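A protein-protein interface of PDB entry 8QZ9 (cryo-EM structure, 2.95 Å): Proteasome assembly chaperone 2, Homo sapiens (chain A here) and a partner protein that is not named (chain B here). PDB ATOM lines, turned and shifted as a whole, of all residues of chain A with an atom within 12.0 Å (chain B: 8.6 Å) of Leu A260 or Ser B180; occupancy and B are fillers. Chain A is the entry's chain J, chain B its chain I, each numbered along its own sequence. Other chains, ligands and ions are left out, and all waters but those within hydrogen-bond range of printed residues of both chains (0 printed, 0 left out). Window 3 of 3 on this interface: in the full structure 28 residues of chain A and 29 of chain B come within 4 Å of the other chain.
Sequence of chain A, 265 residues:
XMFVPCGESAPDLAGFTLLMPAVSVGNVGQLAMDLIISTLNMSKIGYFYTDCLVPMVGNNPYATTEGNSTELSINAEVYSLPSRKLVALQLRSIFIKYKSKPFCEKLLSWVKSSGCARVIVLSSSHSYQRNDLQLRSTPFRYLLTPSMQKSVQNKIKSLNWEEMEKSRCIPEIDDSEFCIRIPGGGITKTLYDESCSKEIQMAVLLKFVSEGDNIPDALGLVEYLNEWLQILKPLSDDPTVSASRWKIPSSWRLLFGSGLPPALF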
ATOM      1  N   ARG A 253      36.884  13.900 -28.319  1.00  0.00           N
ATOM      2  CA  ARG A 253      35.919  14.226 -29.364  1.00  0.00           C
ATOM      3  C   ARG A 253      35.331  15.625 -29.196  1.00  0.00           C
ATOM      4  O   ARG A 253      35.484  16.479 -30.074  1.00  0.00           O
ATOM      5  CB  ARG A 253      34.803  13.178 -29.385  1.00  0.00           C
ATOM      6  CG  ARG A 253      35.133  11.936 -30.189  1.00  0.00           C
ATOM      7  CD  ARG A 253      33.933  11.016 -30.278  1.00  0.00           C
ATOM      8  NE  ARG A 253      32.768  11.694 -30.835  1.00  0.00           N
ATOM      9  CZ  ARG A 253      31.580  11.746 -30.250  1.00  0.00           C
ATOM     10  NH1 ARG A 253      31.361  11.174 -29.077  1.00  0.00           N
ATOM     11  NH2 ARG A 253      30.586  12.387 -30.857  1.00  0.00           N
ATOM     12  N   LEU A 254      34.659  15.873 -28.075  1.00  0.00           N
ATOM     13  CA  LEU A 254      33.924  17.115 -27.846  1.00  0.00           C
ATOM     14  C   LEU A 254      34.508  17.795 -26.613  1.00  0.00           C
ATOM     15  O   LEU A 254      34.039  17.583 -25.493  1.00  0.00           O
ATOM     16  CB  LEU A 254      32.437  16.838 -27.678  1.00  0.00           C
ATOM     17  CG  LEU A 254      31.759  16.104 -28.835  1.00  0.00           C
ATOM     18  CD1 LEU A 254      30.442  15.503 -28.389  1.00  0.00           C
ATOM     19  CD2 LEU A 254      31.544  17.045 -30.004  1.00  0.00           C
ATOM     20  N   PHE A 256      34.656  21.146 -26.242  1.00  0.00           N
ATOM     21  CA  PHE A 256      34.093  22.477 -26.070  1.00  0.00           C
ATOM     22  C   PHE A 256      32.586  22.493 -25.860  1.00  0.00           C
ATOM     23  O   PHE A 256      32.039  23.557 -25.554  1.00  0.00           O
ATOM     24  CB  PHE A 256      34.434  23.368 -27.275  1.00  0.00           C
ATOM     25  CG  PHE A 256      35.714  24.136 -27.121  1.00  0.00           C
ATOM     26  CD1 PHE A 256      35.749  25.304 -26.381  1.00  0.00           C
ATOM     27  CD2 PHE A 256      36.878  23.700 -27.726  1.00  0.00           C
ATOM     28  CE1 PHE A 256      36.922  26.015 -26.240  1.00  0.00           C
ATOM     29  CE2 PHE A 256      38.053  24.408 -27.589  1.00  0.00           C
ATOM     30  CZ  PHE A 256      38.074  25.566 -26.845  1.00  0.00           C
ATOM     31  N   GLY A 257      31.898  21.366 -26.018  1.00  0.00           N
ATOM     32  CA  GLY A 257      30.469  21.303 -25.807  1.00  0.00           C
ATOM     33  C   GLY A 257      29.778  20.543 -26.913  1.00  0.00           C
ATOM     34  O   GLY A 257      30.413  19.900 -27.755  1.00  0.00           O
ATOM     35  N   SER A 258      28.446  20.619 -26.917  1.00  0.00           N
ATOM     36  CA  SER A 258      27.651  19.804 -27.830  1.00  0.00           C
ATOM     37  C   SER A 258      27.530  20.437 -29.215  1.00  0.00           C
ATOM     38  O   SER A 258      27.992  19.868 -30.209  1.00  0.00           O
ATOM     39  CB  SER A 258      26.265  19.557 -27.234  1.00  0.00           C
ATOM     40  OG  SER A 258      26.365  18.972 -25.948  1.00  0.00           O
ATOM     41  N   GLY A 259      26.915  21.610 -29.302  1.00  0.00           N
ATOM     42  CA  GLY A 259      26.663  22.201 -30.604  1.00  0.00           C
ATOM     43  C   GLY A 259      25.863  23.479 -30.481  1.00  0.00           C
ATOM     44  O   GLY A 259      25.584  23.967 -29.381  1.00  0.00           O
ATOM     45  N   LEU A 260      25.492  24.018 -31.648  1.00  0.00           N
ATOM     46  CA  LEU A 260      24.784  25.289 -31.790  1.00  0.00           C
ATOM     47  C   LEU A 260      23.276  25.079 -31.750  1.00  0.00           C
ATOM     48  O   LEU A 260      22.753  24.249 -32.502  1.00  0.00           O
ATOM     49  CB  LEU A 260      25.154  25.971 -33.098  1.00  0.00           C
ATOM     50  CG  LEU A 260      26.581  26.482 -33.262  1.00  0.00           C
ATOM     51  CD1 LEU A 260      26.796  26.974 -34.677  1.00  0.00           C
ATOM     52  CD2 LEU A 260      26.815  27.603 -32.278  1.00  0.00           C
ATOM     53  N   PRO A 261      22.551  25.806 -30.899  1.00  0.00           N
ATOM     54  CA  PRO A 261      21.096  25.811 -31.006  1.00  0.00           C
ATOM     55  C   PRO A 261      20.662  26.483 -32.292  1.00  0.00           C
ATOM     56  O   PRO A 261      21.371  27.358 -32.823  1.00  0.00           O
ATOM     57  CB  PRO A 261      20.651  26.617 -29.771  1.00  0.00           C
ATOM     58  CG  PRO A 261      21.842  26.664 -28.876  1.00  0.00           C
ATOM     59  CD  PRO A 261      23.026  26.632 -29.778  1.00  0.00           C
ATOM     60  N   PRO A 262      19.509  26.114 -32.838  1.00  0.00           N
ATOM     61  CA  PRO A 262      19.062  26.699 -34.104  1.00  0.00           C
ATOM     62  C   PRO A 262      18.514  28.107 -33.908  1.00  0.00           C
ATOM     63  O   PRO A 262      18.267  28.564 -32.792  1.00  0.00           O
ATOM     64  CB  PRO A 262      17.960  25.740 -34.578  1.00  0.00           C
ATOM     65  CG  PRO A 262      17.914  24.618 -33.563  1.00  0.00           C
ATOM     66  CD  PRO A 262      18.544  25.136 -32.319  1.00  0.00           C
ATOM     67  N   ALA A 263      18.335  28.794 -35.038  1.00  0.00           N
ATOM     68  CA  ALA A 263      17.701  30.113 -35.082  1.00  0.00           C
ATOM     69  C   ALA A 263      18.447  31.135 -34.229  1.00  0.00           C
ATOM     70  O   ALA A 263      17.839  31.951 -33.534  1.00  0.00           O
ATOM     71  CB  ALA A 263      16.232  30.031 -34.664  1.00  0.00           C
ATOM     72  N   LEU A 264      19.764  31.094 -34.275  1.00  0.00           N
ATOM     73  CA  LEU A 264      20.551  32.086 -33.555  1.00  0.00           C
ATOM     74  C   LEU A 264      21.590  32.758 -34.440  1.00  0.00           C
ATOM     75  O   LEU A 264      21.853  33.950 -34.270  1.00  0.00           O
ATOM     76  CB  LEU A 264      21.223  31.428 -32.334  1.00  0.00           C
ATOM     77  CG  LEU A 264      21.964  32.286 -31.304  1.00  0.00           C
ATOM     78  CD1 LEU A 264      21.943  31.581 -29.964  1.00  0.00           C
ATOM     79  CD2 LEU A 264      23.397  32.571 -31.705  1.00  0.00           C
ATOM     80  N   PHE A 265      22.183  32.026 -35.377  1.00  0.00           N
ATOM     81  CA  PHE A 265      23.164  32.597 -36.292  1.00  0.00           C
ATOM     82  C   PHE A 265      22.567  32.782 -37.682  1.00  0.00           C
ATOM     83  O   PHE A 265      22.215  31.810 -38.350  1.00  0.00           O
ATOM     84  CB  PHE A 265      24.410  31.716 -36.368  1.00  0.00           C
ATOM     85  CG  PHE A 265      25.436  32.025 -35.320  1.00  0.00           C
ATOM     86  CD1 PHE A 265      26.298  33.094 -35.472  1.00  0.00           C
ATOM     87  CD2 PHE A 265      25.537  31.248 -34.182  1.00  0.00           C
ATOM     88  CE1 PHE A 265      27.238  33.382 -34.509  1.00  0.00           C
ATOM     89  CE2 PHE A 265      26.477  31.533 -33.216  1.00  0.00           C
ATOM     90  CZ  PHE A 265      27.327  32.601 -33.380  1.00  0.00           C
ATOM     91  N   VAL B 172      19.085  16.576 -19.174  1.00  0.00           N
ATOM     92  CA  VAL B 172      19.500  16.319 -20.546  1.00  0.00           C
ATOM     93  C   VAL B 172      20.597  17.275 -20.993  1.00  0.00           C
ATOM     94  O   VAL B 172      21.321  16.977 -21.949  1.00  0.00           O
ATOM     95  CB  VAL B 172      18.283  16.393 -21.488  1.00  0.00           C
ATOM     96  CG1 VAL B 172      17.806  17.827 -21.635  1.00  0.00           C
ATOM     97  CG2 VAL B 172      18.603  15.774 -22.839  1.00  0.00           C
ATOM     98  N   TYR B 175      24.291  15.929 -21.315  1.00  0.00           N
ATOM     99  CA  TYR B 175      24.663  15.000 -22.368  1.00  0.00           C
ATOM    100  C   TYR B 175      25.560  15.684 -23.393  1.00  0.00           C
ATOM    101  O   TYR B 175      25.459  16.890 -23.629  1.00  0.00           O
ATOM    102  CB  TYR B 175      23.414  14.444 -23.053  1.00  0.00           C
ATOM    103  CG  TYR B 175      23.618  13.103 -23.711  1.00  0.00           C
ATOM    104  CD1 TYR B 175      24.140  12.034 -23.002  1.00  0.00           C
ATOM    105  CD2 TYR B 175      23.286  12.906 -25.040  1.00  0.00           C
ATOM    106  CE1 TYR B 175      24.328  10.806 -23.601  1.00  0.00           C
ATOM    107  CE2 TYR B 175      23.471  11.685 -25.648  1.00  0.00           C
ATOM    108  CZ  TYR B 175      23.991  10.638 -24.925  1.00  0.00           C
ATOM    109  OH  TYR B 175      24.176   9.417 -25.528  1.00  0.00           O
ATOM    110  N   LYS B 176      26.448  14.899 -23.997  1.00  0.00           N
ATOM    111  CA  LYS B 176      27.374  15.382 -25.015  1.00  0.00           C
ATOM    112  C   LYS B 176      27.025  14.731 -26.344  1.00  0.00           C
ATOM    113  O   LYS B 176      27.045  13.500 -26.460  1.00  0.00           O
ATOM    114  CB  LYS B 176      28.821  15.077 -24.628  1.00  0.00           C
ATOM    115  CG  LYS B 176      29.273  15.755 -23.351  1.00  0.00           C
ATOM    116  CD  LYS B 176      30.709  16.229 -23.460  1.00  0.00           C
ATOM    117  CE  LYS B 176      31.201  16.784 -22.138  1.00  0.00           C
ATOM    118  NZ  LYS B 176      30.096  17.411 -21.368  1.00  0.00           N
ATOM    119  N   THR B 177      26.718  15.552 -27.345  1.00  0.00           N
ATOM    120  CA  THR B 177      26.286  15.066 -28.645  1.00  0.00           C
ATOM    121  C   THR B 177      26.866  15.970 -29.723  1.00  0.00           C
ATOM    122  O   THR B 177      27.153  17.144 -29.485  1.00  0.00           O
ATOM    123  CB  THR B 177      24.750  15.033 -28.740  1.00  0.00           C
ATOM    124  OG1 THR B 177      24.221  14.332 -27.612  1.00  0.00           O
ATOM    125  CG2 THR B 177      24.294  14.318 -29.999  1.00  0.00           C
ATOM    126  N   SER B 178      27.049  15.408 -30.920  1.00  0.00           N
ATOM    127  CA  SER B 178      27.456  16.225 -32.059  1.00  0.00           C
ATOM    128  C   SER B 178      26.396  17.269 -32.389  1.00  0.00           C
ATOM    129  O   SER B 178      26.722  18.420 -32.698  1.00  0.00           O
ATOM    130  CB  SER B 178      27.731  15.339 -33.272  1.00  0.00           C
ATOM    131  OG  SER B 178      28.572  14.252 -32.928  1.00  0.00           O
ATOM    132  N   GLU B 179      25.125  16.883 -32.333  1.00  0.00           N
ATOM    133  CA  GLU B 179      24.027  17.805 -32.567  1.00  0.00           C
ATOM    134  C   GLU B 179      23.728  18.612 -31.306  1.00  0.00           C
ATOM    135  O   GLU B 179      24.292  18.379 -30.234  1.00  0.00           O
ATOM    136  CB  GLU B 179      22.778  17.049 -33.015  1.00  0.00           C
ATOM    137  CG  GLU B 179      22.908  16.382 -34.371  1.00  0.00           C
ATOM    138  CD  GLU B 179      23.425  14.963 -34.271  1.00  0.00           C
ATOM    139  OE1 GLU B 179      23.336  14.377 -33.173  1.00  0.00           O
ATOM    140  OE2 GLU B 179      23.919  14.433 -35.288  1.00  0.00           O
ATOM    141  N   SER B 180      22.825  19.578 -31.446  1.00  0.00           N
ATOM    142  CA  SER B 180      22.402  20.369 -30.301  1.00  0.00           C
ATOM    143  C   SER B 180      21.601  19.512 -29.330  1.00  0.00           C
ATOM    144  O   SER B 180      20.862  18.608 -29.727  1.00  0.00           O
ATOM    145  CB  SER B 180      21.568  21.566 -30.755  1.00  0.00           C
ATOM    146  OG  SER B 180      20.369  21.143 -31.379  1.00  0.00           O
ATOM    147  N   THR B 181      21.756  19.807 -28.037  1.00  0.00           N
ATOM    148  CA  THR B 181      21.106  19.010 -27.002  1.00  0.00           C
ATOM    149  C   THR B 181      19.590  19.147 -27.020  1.00  0.00           C
ATOM    150  O   THR B 181      18.902  18.322 -26.411  1.00  0.00           O
ATOM    151  CB  THR B 181      21.642  19.397 -25.623  1.00  0.00           C
ATOM    152  OG1 THR B 181      21.113  18.503 -24.637  1.00  0.00           O
ATOM    153  CG2 THR B 181      21.241  20.820 -25.275  1.00  0.00           C
ATOM    154  N   GLY B 182      19.054  20.162 -27.696  1.00  0.00           N
ATOM    155  CA  GLY B 182      17.616  20.323 -27.785  1.00  0.00           C
ATOM    156  C   GLY B 182      16.936  19.481 -28.840  1.00  0.00           C
ATOM    157  O   GLY B 182      15.705  19.479 -28.911  1.00  0.00           O
ATOM    158  N   SER B 183      17.705  18.766 -29.660  1.00  0.00           N
ATOM    159  CA  SER B 183      17.145  17.931 -30.713  1.00  0.00           C
ATOM    160  C   SER B 183      16.926  16.487 -30.284  1.00  0.00           C
ATOM    161  O   SER B 183      16.318  15.720 -31.038  1.00  0.00           O
ATOM    162  CB  SER B 183      18.056  17.958 -31.944  1.00  0.00           C
ATOM    163  OG  SER B 183      18.190  19.273 -32.452  1.00  0.00           O
ATOM    164  N   LEU B 184      17.402  16.101 -29.109  1.00  0.00           N
ATOM    165  CA  LEU B 184      17.279  14.722 -28.671  1.00  0.00           C
ATOM    166  C   LEU B 184      15.845  14.411 -28.246  1.00  0.00           C
ATOM    167  O   LEU B 184      15.145  15.276 -27.714  1.00  0.00           O
ATOM    168  CB  LEU B 184      18.231  14.449 -27.514  1.00  0.00           C
ATOM    169  CG  LEU B 184      19.686  14.840 -27.770  1.00  0.00           C
ATOM    170  CD1 LEU B 184      20.513  14.686 -26.510  1.00  0.00           C
ATOM    171  CD2 LEU B 184      20.266  14.009 -28.900  1.00  0.00           C
ATOM    172  N   PRO B 185      15.384  13.180 -28.474  1.00  0.00           N
ATOM    173  CA  PRO B 185      14.023  12.785 -28.058  1.00  0.00           C
ATOM    174  C   PRO B 185      13.977  12.310 -26.608  1.00  0.00           C
ATOM    175  O   PRO B 185      13.766  11.129 -26.302  1.00  0.00           O
ATOM    176  CB  PRO B 185      13.690  11.673 -29.054  1.00  0.00           C
ATOM    177  CG  PRO B 185      15.007  11.031 -29.328  1.00  0.00           C
ATOM    178  CD  PRO B 185      16.063  12.106 -29.219  1.00  0.00           C
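Of chain B, only Ser B180 (3.4 Å) comes within 4 Å of Leu A260. Ser B180 touches one residue of chain A. No residue of chain B comes within 4 Å of Gly A259. Pro A261 touches none of the printed residues of chain B. Of chain A, only Leu A254 (3.8 Å) and Ser A258 (2.9 Å) come within 4 Å of Thr B177. Of chain A, only Ser A258 comes within 4 Å of Glu B179. No residue of chain A comes within 4 Å of Thr B181. No residue of chain A comes within 4 Å of Gly B182. Printed residues of chain B within 4 Å of Arg A253: Ser B178 (3.4 Å). Of the printed residues of chain A, Tyr B175 touches Ser A258 (3.2 Å). Of the printed residues of chain A, Lys B176 touches Ser A258 (3.8 Å). Phe A265 touches none of the printed residues of chain B.
The guanidinium group (NH2) of Arg A253 sits at hydrogen-bond distance from the side-chain hydroxyl (OG) of Ser B178 (3.4 Å). O of Tyr B175 sits at hydrogen-bond distance from OG of Ser A258 (3.2 Å). The backbone carbonyl oxygen (O) of Ser A258 lies close to the backbone carbonyl oxygen (O) of Thr B177 (2.9 Å). The backbone carbonyl oxygen (O) of Ser A258 lies close to the backbone carbonyl oxygen (O) of Ser B178, 3.1 Å away.
Thr B177 touches Leu A254. CA of Lys B176 touches OG of Ser A258, 3.8 Å away. Ser A258 touches Glu B179 (CB to O, 3.8 Å). Leu A260 touches Ser B180 (O to CB, 3.4 Å).
The side-chain hydroxyl (OG) of Ser B180 is in hydrogen-bond range of the side-chain hydroxyl (OG) of Ser B183.
Of the 12 printed residues of chain A, 4 touch a printed residue of chain B. Printed residues of chain A that touch a printed residue of chain B: Arg A253, Leu A254, Ser A258 and Leu A260. Of the 12 printed residues of chain B, 6 touch a printed residue of chain A. Printed residues of chain B that touch a printed residue of chain A: Tyr B175, Lys B176, Thr B177, Ser B178, Glu B179 and Ser B180. Among the printed residues, 8 pairs touch across the chains.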
